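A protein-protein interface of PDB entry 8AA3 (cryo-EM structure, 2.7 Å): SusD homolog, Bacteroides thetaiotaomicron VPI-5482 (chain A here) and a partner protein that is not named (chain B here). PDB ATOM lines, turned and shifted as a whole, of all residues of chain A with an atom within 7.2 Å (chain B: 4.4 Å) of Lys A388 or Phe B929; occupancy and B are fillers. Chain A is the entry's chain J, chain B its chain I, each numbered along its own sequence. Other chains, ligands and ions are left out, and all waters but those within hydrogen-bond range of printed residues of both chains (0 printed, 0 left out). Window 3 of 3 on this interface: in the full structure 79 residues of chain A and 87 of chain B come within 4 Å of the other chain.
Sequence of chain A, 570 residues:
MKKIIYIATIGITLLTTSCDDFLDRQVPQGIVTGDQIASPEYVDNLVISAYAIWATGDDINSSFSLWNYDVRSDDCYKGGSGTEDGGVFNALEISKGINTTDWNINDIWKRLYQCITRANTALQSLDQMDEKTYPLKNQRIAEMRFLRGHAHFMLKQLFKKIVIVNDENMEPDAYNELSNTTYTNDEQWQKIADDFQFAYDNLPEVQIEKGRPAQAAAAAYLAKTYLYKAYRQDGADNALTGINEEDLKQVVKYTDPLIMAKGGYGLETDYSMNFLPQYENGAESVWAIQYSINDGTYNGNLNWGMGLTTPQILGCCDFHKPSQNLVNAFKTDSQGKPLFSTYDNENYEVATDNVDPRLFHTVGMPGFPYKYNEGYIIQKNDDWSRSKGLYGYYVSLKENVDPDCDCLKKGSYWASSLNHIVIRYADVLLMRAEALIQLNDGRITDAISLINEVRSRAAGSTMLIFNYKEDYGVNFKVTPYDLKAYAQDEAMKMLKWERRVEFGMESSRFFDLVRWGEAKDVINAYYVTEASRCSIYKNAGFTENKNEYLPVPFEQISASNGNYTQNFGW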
ATOM      1  N   GLY A  80      13.277 -27.079 -24.170  1.00  0.00           N
ATOM      2  CA  GLY A  80      13.507 -26.259 -22.997  1.00  0.00           C
ATOM      3  C   GLY A  80      12.724 -24.961 -23.044  1.00  0.00           C
ATOM      4  O   GLY A  80      11.938 -24.692 -23.957  1.00  0.00           O
ATOM      5  N   SER A  81      12.955 -24.143 -22.013  1.00  0.00           N
ATOM      6  CA  SER A  81      12.277 -22.854 -21.925  1.00  0.00           C
ATOM      7  C   SER A  81      12.688 -21.932 -23.066  1.00  0.00           C
ATOM      8  O   SER A  81      11.850 -21.223 -23.635  1.00  0.00           O
ATOM      9  CB  SER A  81      12.568 -22.200 -20.574  1.00  0.00           C
ATOM     10  OG  SER A  81      13.948 -22.268 -20.262  1.00  0.00           O
ATOM     11  N   ASP A 318      10.689 -31.218 -21.686  1.00  0.00           N
ATOM     12  CA  ASP A 318      10.267 -30.898 -23.050  1.00  0.00           C
ATOM     13  C   ASP A 318      11.458 -30.490 -23.921  1.00  0.00           C
ATOM     14  O   ASP A 318      11.557 -29.359 -24.404  1.00  0.00           O
ATOM     15  CB  ASP A 318       9.184 -29.815 -23.056  1.00  0.00           C
ATOM     16  CG  ASP A 318       8.504 -29.679 -24.407  1.00  0.00           C
ATOM     17  OD1 ASP A 318       8.022 -30.703 -24.939  1.00  0.00           O
ATOM     18  OD2 ASP A 318       8.472 -28.553 -24.945  1.00  0.00           O
ATOM     19  N   ASN A 381      -0.711 -25.248 -26.872  1.00  0.00           N
ATOM     20  CA  ASN A 381      -0.834 -24.391 -25.702  1.00  0.00           C
ATOM     21  C   ASN A 381       0.401 -24.568 -24.830  1.00  0.00           C
ATOM     22  O   ASN A 381       1.321 -25.322 -25.162  1.00  0.00           O
ATOM     23  CB  ASN A 381      -2.119 -24.695 -24.921  1.00  0.00           C
ATOM     24  CG  ASN A 381      -2.349 -26.183 -24.726  1.00  0.00           C
ATOM     25  OD1 ASN A 381      -1.403 -26.970 -24.677  1.00  0.00           O
ATOM     26  ND2 ASN A 381      -3.612 -26.574 -24.610  1.00  0.00           N
ATOM     27  N   ASP A 382       0.420 -23.860 -23.699  1.00  0.00           N
ATOM     28  CA  ASP A 382       1.544 -23.936 -22.774  1.00  0.00           C
ATOM     29  C   ASP A 382       1.613 -25.265 -22.034  1.00  0.00           C
ATOM     30  O   ASP A 382       2.646 -25.558 -21.422  1.00  0.00           O
ATOM     31  CB  ASP A 382       1.471 -22.789 -21.765  1.00  0.00           C
ATOM     32  CG  ASP A 382       1.564 -21.427 -22.425  1.00  0.00           C
ATOM     33  OD1 ASP A 382       1.424 -21.353 -23.664  1.00  0.00           O
ATOM     34  OD2 ASP A 382       1.775 -20.428 -21.703  1.00  0.00           O
ATOM     35  N   SER A 385       4.055 -27.226 -24.787  1.00  0.00           N
ATOM     36  CA  SER A 385       5.297 -26.601 -25.219  1.00  0.00           C
ATOM     37  C   SER A 385       5.833 -25.711 -24.106  1.00  0.00           C
ATOM     38  O   SER A 385       5.121 -24.828 -23.615  1.00  0.00           O
ATOM     39  CB  SER A 385       5.086 -25.785 -26.495  1.00  0.00           C
ATOM     40  OG  SER A 385       6.286 -25.148 -26.899  1.00  0.00           O
ATOM     41  N   ARG A 386       7.084 -25.946 -23.714  1.00  0.00           N
ATOM     42  CA  ARG A 386       7.734 -25.159 -22.676  1.00  0.00           C
ATOM     43  C   ARG A 386       8.360 -23.875 -23.207  1.00  0.00           C
ATOM     44  O   ARG A 386       8.722 -23.003 -22.409  1.00  0.00           O
ATOM     45  CB  ARG A 386       8.808 -26.003 -21.977  1.00  0.00           C
ATOM     46  CG  ARG A 386       9.177 -25.531 -20.580  1.00  0.00           C
ATOM     47  CD  ARG A 386      10.096 -26.531 -19.896  1.00  0.00           C
ATOM     48  NE  ARG A 386      11.155 -25.882 -19.132  1.00  0.00           N
ATOM     49  CZ  ARG A 386      12.400 -26.328 -19.054  1.00  0.00           C
ATOM     50  NH1 ARG A 386      12.782 -27.425 -19.686  1.00  0.00           N
ATOM     51  NH2 ARG A 386      13.284 -25.658 -18.322  1.00  0.00           N
ATOM     52  N   SER A 387       8.488 -23.732 -24.525  1.00  0.00           N
ATOM     53  CA  SER A 387       9.094 -22.556 -25.133  1.00  0.00           C
ATOM     54  C   SER A 387       8.062 -21.557 -25.638  1.00  0.00           C
ATOM     55  O   SER A 387       8.432 -20.590 -26.311  1.00  0.00           O
ATOM     56  CB  SER A 387      10.018 -22.974 -26.278  1.00  0.00           C
ATOM     57  OG  SER A 387       9.279 -23.267 -27.451  1.00  0.00           O
ATOM     58  N   LYS A 388       6.780 -21.769 -25.326  1.00  0.00           N
ATOM     59  CA  LYS A 388       5.698 -20.882 -25.757  1.00  0.00           C
ATOM     60  C   LYS A 388       5.669 -20.733 -27.277  1.00  0.00           C
ATOM     61  O   LYS A 388       5.459 -19.641 -27.810  1.00  0.00           O
ATOM     62  CB  LYS A 388       5.799 -19.513 -25.077  1.00  0.00           C
ATOM     63  CG  LYS A 388       5.718 -19.568 -23.561  1.00  0.00           C
ATOM     64  CD  LYS A 388       5.919 -18.193 -22.947  1.00  0.00           C
ATOM     65  CE  LYS A 388       5.800 -18.241 -21.433  1.00  0.00           C
ATOM     66  NZ  LYS A 388       6.893 -19.041 -20.815  1.00  0.00           N
ATOM     67  N   GLY A 389       5.884 -21.842 -27.982  1.00  0.00           N
ATOM     68  CA  GLY A 389       5.852 -21.850 -29.428  1.00  0.00           C
ATOM     69  C   GLY A 389       7.143 -21.457 -30.110  1.00  0.00           C
ATOM     70  O   GLY A 389       7.187 -21.442 -31.347  1.00  0.00           O
ATOM     71  N   LEU A 390       8.192 -21.131 -29.351  1.00  0.00           N
ATOM     72  CA  LEU A 390       9.465 -20.766 -29.968  1.00  0.00           C
ATOM     73  C   LEU A 390      10.068 -21.940 -30.727  1.00  0.00           C
ATOM     74  O   LEU A 390      10.592 -21.770 -31.834  1.00  0.00           O
ATOM     75  CB  LEU A 390      10.436 -20.257 -28.901  1.00  0.00           C
ATOM     76  CG  LEU A 390      11.897 -20.088 -29.324  1.00  0.00           C
ATOM     77  CD1 LEU A 390      12.028 -19.020 -30.399  1.00  0.00           C
ATOM     78  CD2 LEU A 390      12.770 -19.756 -28.124  1.00  0.00           C
ATOM     79  N   TYR A 391      10.002 -23.140 -30.151  1.00  0.00           N
ATOM     80  CA  TYR A 391      10.561 -24.338 -30.763  1.00  0.00           C
ATOM     81  C   TYR A 391       9.489 -25.232 -31.379  1.00  0.00           C
ATOM     82  O   TYR A 391       9.763 -26.398 -31.683  1.00  0.00           O
ATOM     83  CB  TYR A 391      11.378 -25.121 -29.735  1.00  0.00           C
ATOM     84  CG  TYR A 391      12.684 -24.456 -29.362  1.00  0.00           C
ATOM     85  CD1 TYR A 391      13.715 -24.339 -30.285  1.00  0.00           C
ATOM     86  CD2 TYR A 391      12.886 -23.947 -28.086  1.00  0.00           C
ATOM     87  CE1 TYR A 391      14.910 -23.732 -29.947  1.00  0.00           C
ATOM     88  CE2 TYR A 391      14.077 -23.339 -27.739  1.00  0.00           C
ATOM     89  CZ  TYR A 391      15.085 -23.234 -28.674  1.00  0.00           C
ATOM     90  OH  TYR A 391      16.274 -22.629 -28.335  1.00  0.00           O
ATOM     91  N   GLY A 392       8.281 -24.714 -31.565  1.00  0.00           N
ATOM     92  CA  GLY A 392       7.207 -25.497 -32.140  1.00  0.00           C
ATOM     93  C   GLY A 392       6.375 -26.209 -31.093  1.00  0.00           C
ATOM     94  O   GLY A 392       6.443 -25.938 -29.891  1.00  0.00           O
ATOM     95  N   TYR A 393       5.561 -27.148 -31.581  1.00  0.00           N
ATOM     96  CA  TYR A 393       4.680 -27.927 -30.722  1.00  0.00           C
ATOM     97  C   TYR A 393       4.764 -29.425 -30.996  1.00  0.00           C
ATOM     98  O   TYR A 393       3.914 -30.178 -30.508  1.00  0.00           O
ATOM     99  CB  TYR A 393       3.229 -27.454 -30.871  1.00  0.00           C
ATOM    100  CG  TYR A 393       3.015 -26.007 -30.487  1.00  0.00           C
ATOM    101  CD1 TYR A 393       2.748 -25.649 -29.173  1.00  0.00           C
ATOM    102  CD2 TYR A 393       3.081 -24.998 -31.440  1.00  0.00           C
ATOM    103  CE1 TYR A 393       2.553 -24.328 -28.818  1.00  0.00           C
ATOM    104  CE2 TYR A 393       2.888 -23.675 -31.095  1.00  0.00           C
ATOM    105  CZ  TYR A 393       2.624 -23.345 -29.782  1.00  0.00           C
ATOM    106  OH  TYR A 393       2.430 -22.028 -29.433  1.00  0.00           O
ATOM    107  N   TYR B 262       7.771  -6.482 -13.006  1.00  0.00           N
ATOM    108  CA  TYR B 262       8.058  -7.642 -13.846  1.00  0.00           C
ATOM    109  C   TYR B 262       7.418  -7.499 -15.221  1.00  0.00           C
ATOM    110  O   TYR B 262       8.051  -7.788 -16.244  1.00  0.00           O
ATOM    111  CB  TYR B 262       7.572  -8.916 -13.155  1.00  0.00           C
ATOM    112  CG  TYR B 262       7.836 -10.191 -13.923  1.00  0.00           C
ATOM    113  CD1 TYR B 262       9.060 -10.841 -13.830  1.00  0.00           C
ATOM    114  CD2 TYR B 262       6.855 -10.754 -14.729  1.00  0.00           C
ATOM    115  CE1 TYR B 262       9.302 -12.009 -14.528  1.00  0.00           C
ATOM    116  CE2 TYR B 262       7.088 -11.919 -15.429  1.00  0.00           C
ATOM    117  CZ  TYR B 262       8.312 -12.542 -15.324  1.00  0.00           C
ATOM    118  OH  TYR B 262       8.544 -13.705 -16.021  1.00  0.00           O
ATOM    119  N   MET B 266       9.428  -7.238 -18.767  1.00  0.00           N
ATOM    120  CA  MET B 266       9.156  -8.162 -19.864  1.00  0.00           C
ATOM    121  C   MET B 266       8.758  -7.412 -21.130  1.00  0.00           C
ATOM    122  O   MET B 266       9.203  -7.758 -22.231  1.00  0.00           O
ATOM    123  CB  MET B 266       8.066  -9.155 -19.457  1.00  0.00           C
ATOM    124  CG  MET B 266       7.790 -10.229 -20.496  1.00  0.00           C
ATOM    125  SD  MET B 266       6.737 -11.552 -19.871  1.00  0.00           S
ATOM    126  CE  MET B 266       5.189 -10.679 -19.657  1.00  0.00           C
ATOM    127  N   TYR B 270      10.747  -7.410 -24.679  1.00  0.00           N
ATOM    128  CA  TYR B 270      10.066  -7.776 -25.916  1.00  0.00           C
ATOM    129  C   TYR B 270      10.206  -6.689 -26.975  1.00  0.00           C
ATOM    130  O   TYR B 270      10.478  -6.986 -28.144  1.00  0.00           O
ATOM    131  CB  TYR B 270       8.591  -8.066 -25.637  1.00  0.00           C
ATOM    132  CG  TYR B 270       8.278  -9.532 -25.443  1.00  0.00           C
ATOM    133  CD1 TYR B 270       8.109 -10.377 -26.532  1.00  0.00           C
ATOM    134  CD2 TYR B 270       8.149 -10.072 -24.169  1.00  0.00           C
ATOM    135  CE1 TYR B 270       7.822 -11.718 -26.359  1.00  0.00           C
ATOM    136  CE2 TYR B 270       7.862 -11.411 -23.986  1.00  0.00           C
ATOM    137  CZ  TYR B 270       7.700 -12.230 -25.085  1.00  0.00           C
ATOM    138  OH  TYR B 270       7.415 -13.564 -24.908  1.00  0.00           O
ATOM    139  N   ASN B 280       3.471 -12.799 -25.113  1.00  0.00           N
ATOM    140  CA  ASN B 280       4.174 -13.385 -23.977  1.00  0.00           C
ATOM    141  C   ASN B 280       3.453 -14.598 -23.405  1.00  0.00           C
ATOM    142  O   ASN B 280       4.101 -15.449 -22.786  1.00  0.00           O
ATOM    143  CB  ASN B 280       4.373 -12.334 -22.884  1.00  0.00           C
ATOM    144  CG  ASN B 280       3.061 -11.763 -22.378  1.00  0.00           C
ATOM    145  OD1 ASN B 280       2.532 -12.205 -21.358  1.00  0.00           O
ATOM    146  ND2 ASN B 280       2.532 -10.774 -23.087  1.00  0.00           N
ATOM    147  N   LEU B 282       1.574 -14.897 -20.874  1.00  0.00           N
ATOM    148  CA  LEU B 282       1.665 -14.921 -19.419  1.00  0.00           C
ATOM    149  C   LEU B 282       0.534 -14.136 -18.765  1.00  0.00           C
ATOM    150  O   LEU B 282       0.626 -13.790 -17.583  1.00  0.00           O
ATOM    151  CB  LEU B 282       3.021 -14.381 -18.959  1.00  0.00           C
ATOM    152  CG  LEU B 282       4.199 -15.357 -19.005  1.00  0.00           C
ATOM    153  CD1 LEU B 282       5.366 -14.828 -18.185  1.00  0.00           C
ATOM    154  CD2 LEU B 282       3.779 -16.735 -18.515  1.00  0.00           C
ATOM    155  N   GLY B 428       2.682 -21.286 -18.616  1.00  0.00           N
ATOM    156  CA  GLY B 428       3.999 -20.920 -19.089  1.00  0.00           C
ATOM    157  C   GLY B 428       4.933 -20.316 -18.068  1.00  0.00           C
ATOM    158  O   GLY B 428       6.048 -19.920 -18.426  1.00  0.00           O
ATOM    159  N   PRO B 430       7.702 -20.015 -15.095  1.00  0.00           N
ATOM    160  CA  PRO B 430       8.912 -20.828 -14.936  1.00  0.00           C
ATOM    161  C   PRO B 430       8.761 -21.877 -13.844  1.00  0.00           C
ATOM    162  O   PRO B 430       8.026 -21.699 -12.872  1.00  0.00           O
ATOM    163  CB  PRO B 430       9.986 -19.796 -14.575  1.00  0.00           C
ATOM    164  CG  PRO B 430       9.232 -18.655 -13.989  1.00  0.00           C
ATOM    165  CD  PRO B 430       7.944 -18.602 -14.760  1.00  0.00           C
ATOM    166  N   GLY B 928      14.136 -19.086 -18.491  1.00  0.00           N
ATOM    167  CA  GLY B 928      13.691 -17.728 -18.712  1.00  0.00           C
ATOM    168  C   GLY B 928      12.487 -17.355 -17.863  1.00  0.00           C
ATOM    169  O   GLY B 928      11.945 -18.156 -17.104  1.00  0.00           O
ATOM    170  N   PHE B 929      12.079 -16.092 -18.006  1.00  0.00           N
ATOM    171  CA  PHE B 929      10.906 -15.541 -17.322  1.00  0.00           C
ATOM    172  C   PHE B 929      11.036 -15.618 -15.803  1.00  0.00           C
ATOM    173  O   PHE B 929      10.038 -15.735 -15.090  1.00  0.00           O
ATOM    174  CB  PHE B 929       9.618 -16.232 -17.783  1.00  0.00           C
ATOM    175  CG  PHE B 929       9.284 -15.993 -19.228  1.00  0.00           C
ATOM    176  CD1 PHE B 929       8.747 -14.784 -19.636  1.00  0.00           C
ATOM    177  CD2 PHE B 929       9.506 -16.978 -20.176  1.00  0.00           C
ATOM    178  CE1 PHE B 929       8.438 -14.560 -20.965  1.00  0.00           C
ATOM    179  CE2 PHE B 929       9.199 -16.760 -21.506  1.00  0.00           C
ATOM    180  CZ  PHE B 929       8.664 -15.549 -21.901  1.00  0.00           C
ATOM    181  N   LEU B 930      12.262 -15.543 -15.294  1.00  0.00           N
ATOM    182  CA  LEU B 930      12.493 -15.551 -13.859  1.00  0.00           C
ATOM    183  C   LEU B 930      12.454 -14.132 -13.300  1.00  0.00           C
ATOM    184  O   LEU B 930      12.679 -13.149 -14.009  1.00  0.00           O
ATOM    185  CB  LEU B 930      13.837 -16.201 -13.526  1.00  0.00           C
ATOM    186  CG  LEU B 930      13.988 -17.696 -13.801  1.00  0.00           C
ATOM    187  CD1 LEU B 930      15.406 -18.144 -13.490  1.00  0.00           C
ATOM    188  CD2 LEU B 930      12.984 -18.491 -12.985  1.00  0.00           C
ATOM    189  N   ASN B 931      12.158 -14.040 -12.006  1.00  0.00           N
ATOM    190  CA  ASN B 931      12.164 -12.750 -11.332  1.00  0.00           C
ATOM    191  C   ASN B 931      13.591 -12.234 -11.198  1.00  0.00           C
ATOM    192  O   ASN B 931      14.517 -12.990 -10.889  1.00  0.00           O
ATOM    193  CB  ASN B 931      11.511 -12.868  -9.955  1.00  0.00           C
ATOM    194  CG  ASN B 931      10.822 -11.589  -9.526  1.00  0.00           C
ATOM    195  OD1 ASN B 931      10.277 -10.856 -10.351  1.00  0.00           O
ATOM    196  ND2 ASN B 931      10.840 -11.316  -8.226  1.00  0.00           N
ATOM    197  N   ARG B 954      15.636 -11.098 -24.680  1.00  0.00           N
ATOM    198  CA  ARG B 954      15.144 -12.435 -24.373  1.00  0.00           C
ATOM    199  C   ARG B 954      16.077 -13.541 -24.845  1.00  0.00           C
ATOM    200  O   ARG B 954      15.992 -14.660 -24.330  1.00  0.00           O
ATOM    201  CB  ARG B 954      13.759 -12.648 -24.997  1.00  0.00           C
ATOM    202  CG  ARG B 954      12.686 -11.714 -24.462  1.00  0.00           C
ATOM    203  CD  ARG B 954      11.295 -12.290 -24.669  1.00  0.00           C
ATOM    204  NE  ARG B 954      11.201 -13.069 -25.898  1.00  0.00           N
ATOM    205  CZ  ARG B 954      10.834 -14.342 -25.952  1.00  0.00           C
ATOM    206  NH1 ARG B 954      10.520 -15.017 -24.859  1.00  0.00           N
ATOM    207  NH2 ARG B 954      10.782 -14.952 -27.132  1.00  0.00           N
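Among the printed residues, merely in contact across the chains: Lys A388 with Asn B280, Lys A388 with Phe B929, Ser A81 with Gly B928 and Lys A388 with Leu B282.
The backbone NH (N) of Leu B282 sits at hydrogen-bond distance from the side-chain amide oxygen (OD1) of Asn B280. O of Phe B929 sits at hydrogen-bond distance from OH of Tyr B262 (2.7 Å).
N of Gly B428 lies within hydrogen-bond range of OD2 of Asp A382. The side-chain amino group (NZ) of Lys A388 sits at hydrogen-bond distance from the backbone carbonyl oxygen (O) of Gly B428.
Printed residues of chain A that touch a printed residue of chain B: Ser A81, Asp A382 and Lys A388. Along chain A the printed residues that touch a printed residue of chain B span positions 81 to 388. Printed residues of chain B that touch a printed residue of chain A: Asn B280, Leu B282, Gly B428, Gly B928 and Phe B929. Among the printed residues, no Asp or Glu carboxylate lies within 4 Å of a Lys or Arg side-chain nitrogen of the other chain.
Lys A388 touches just these residues of chain B: Asn B280, Leu B282, Gly B428 and Phe B929. Phe B929 touches one residue of chain A. Printed residues of chain A within 4 Å of Leu B282: Lys A388 (3.9 Å). Of the printed residues of chain B, Ser A81 touches Gly B928 (3.6 Å). Gly A392 touches none of the printed residues of chain B. Asn A381 touches none of the printed residues of chain B. The nearest printed residue of chain B that does not touch Lys A388 is Tyr B270 (5.2 Å).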
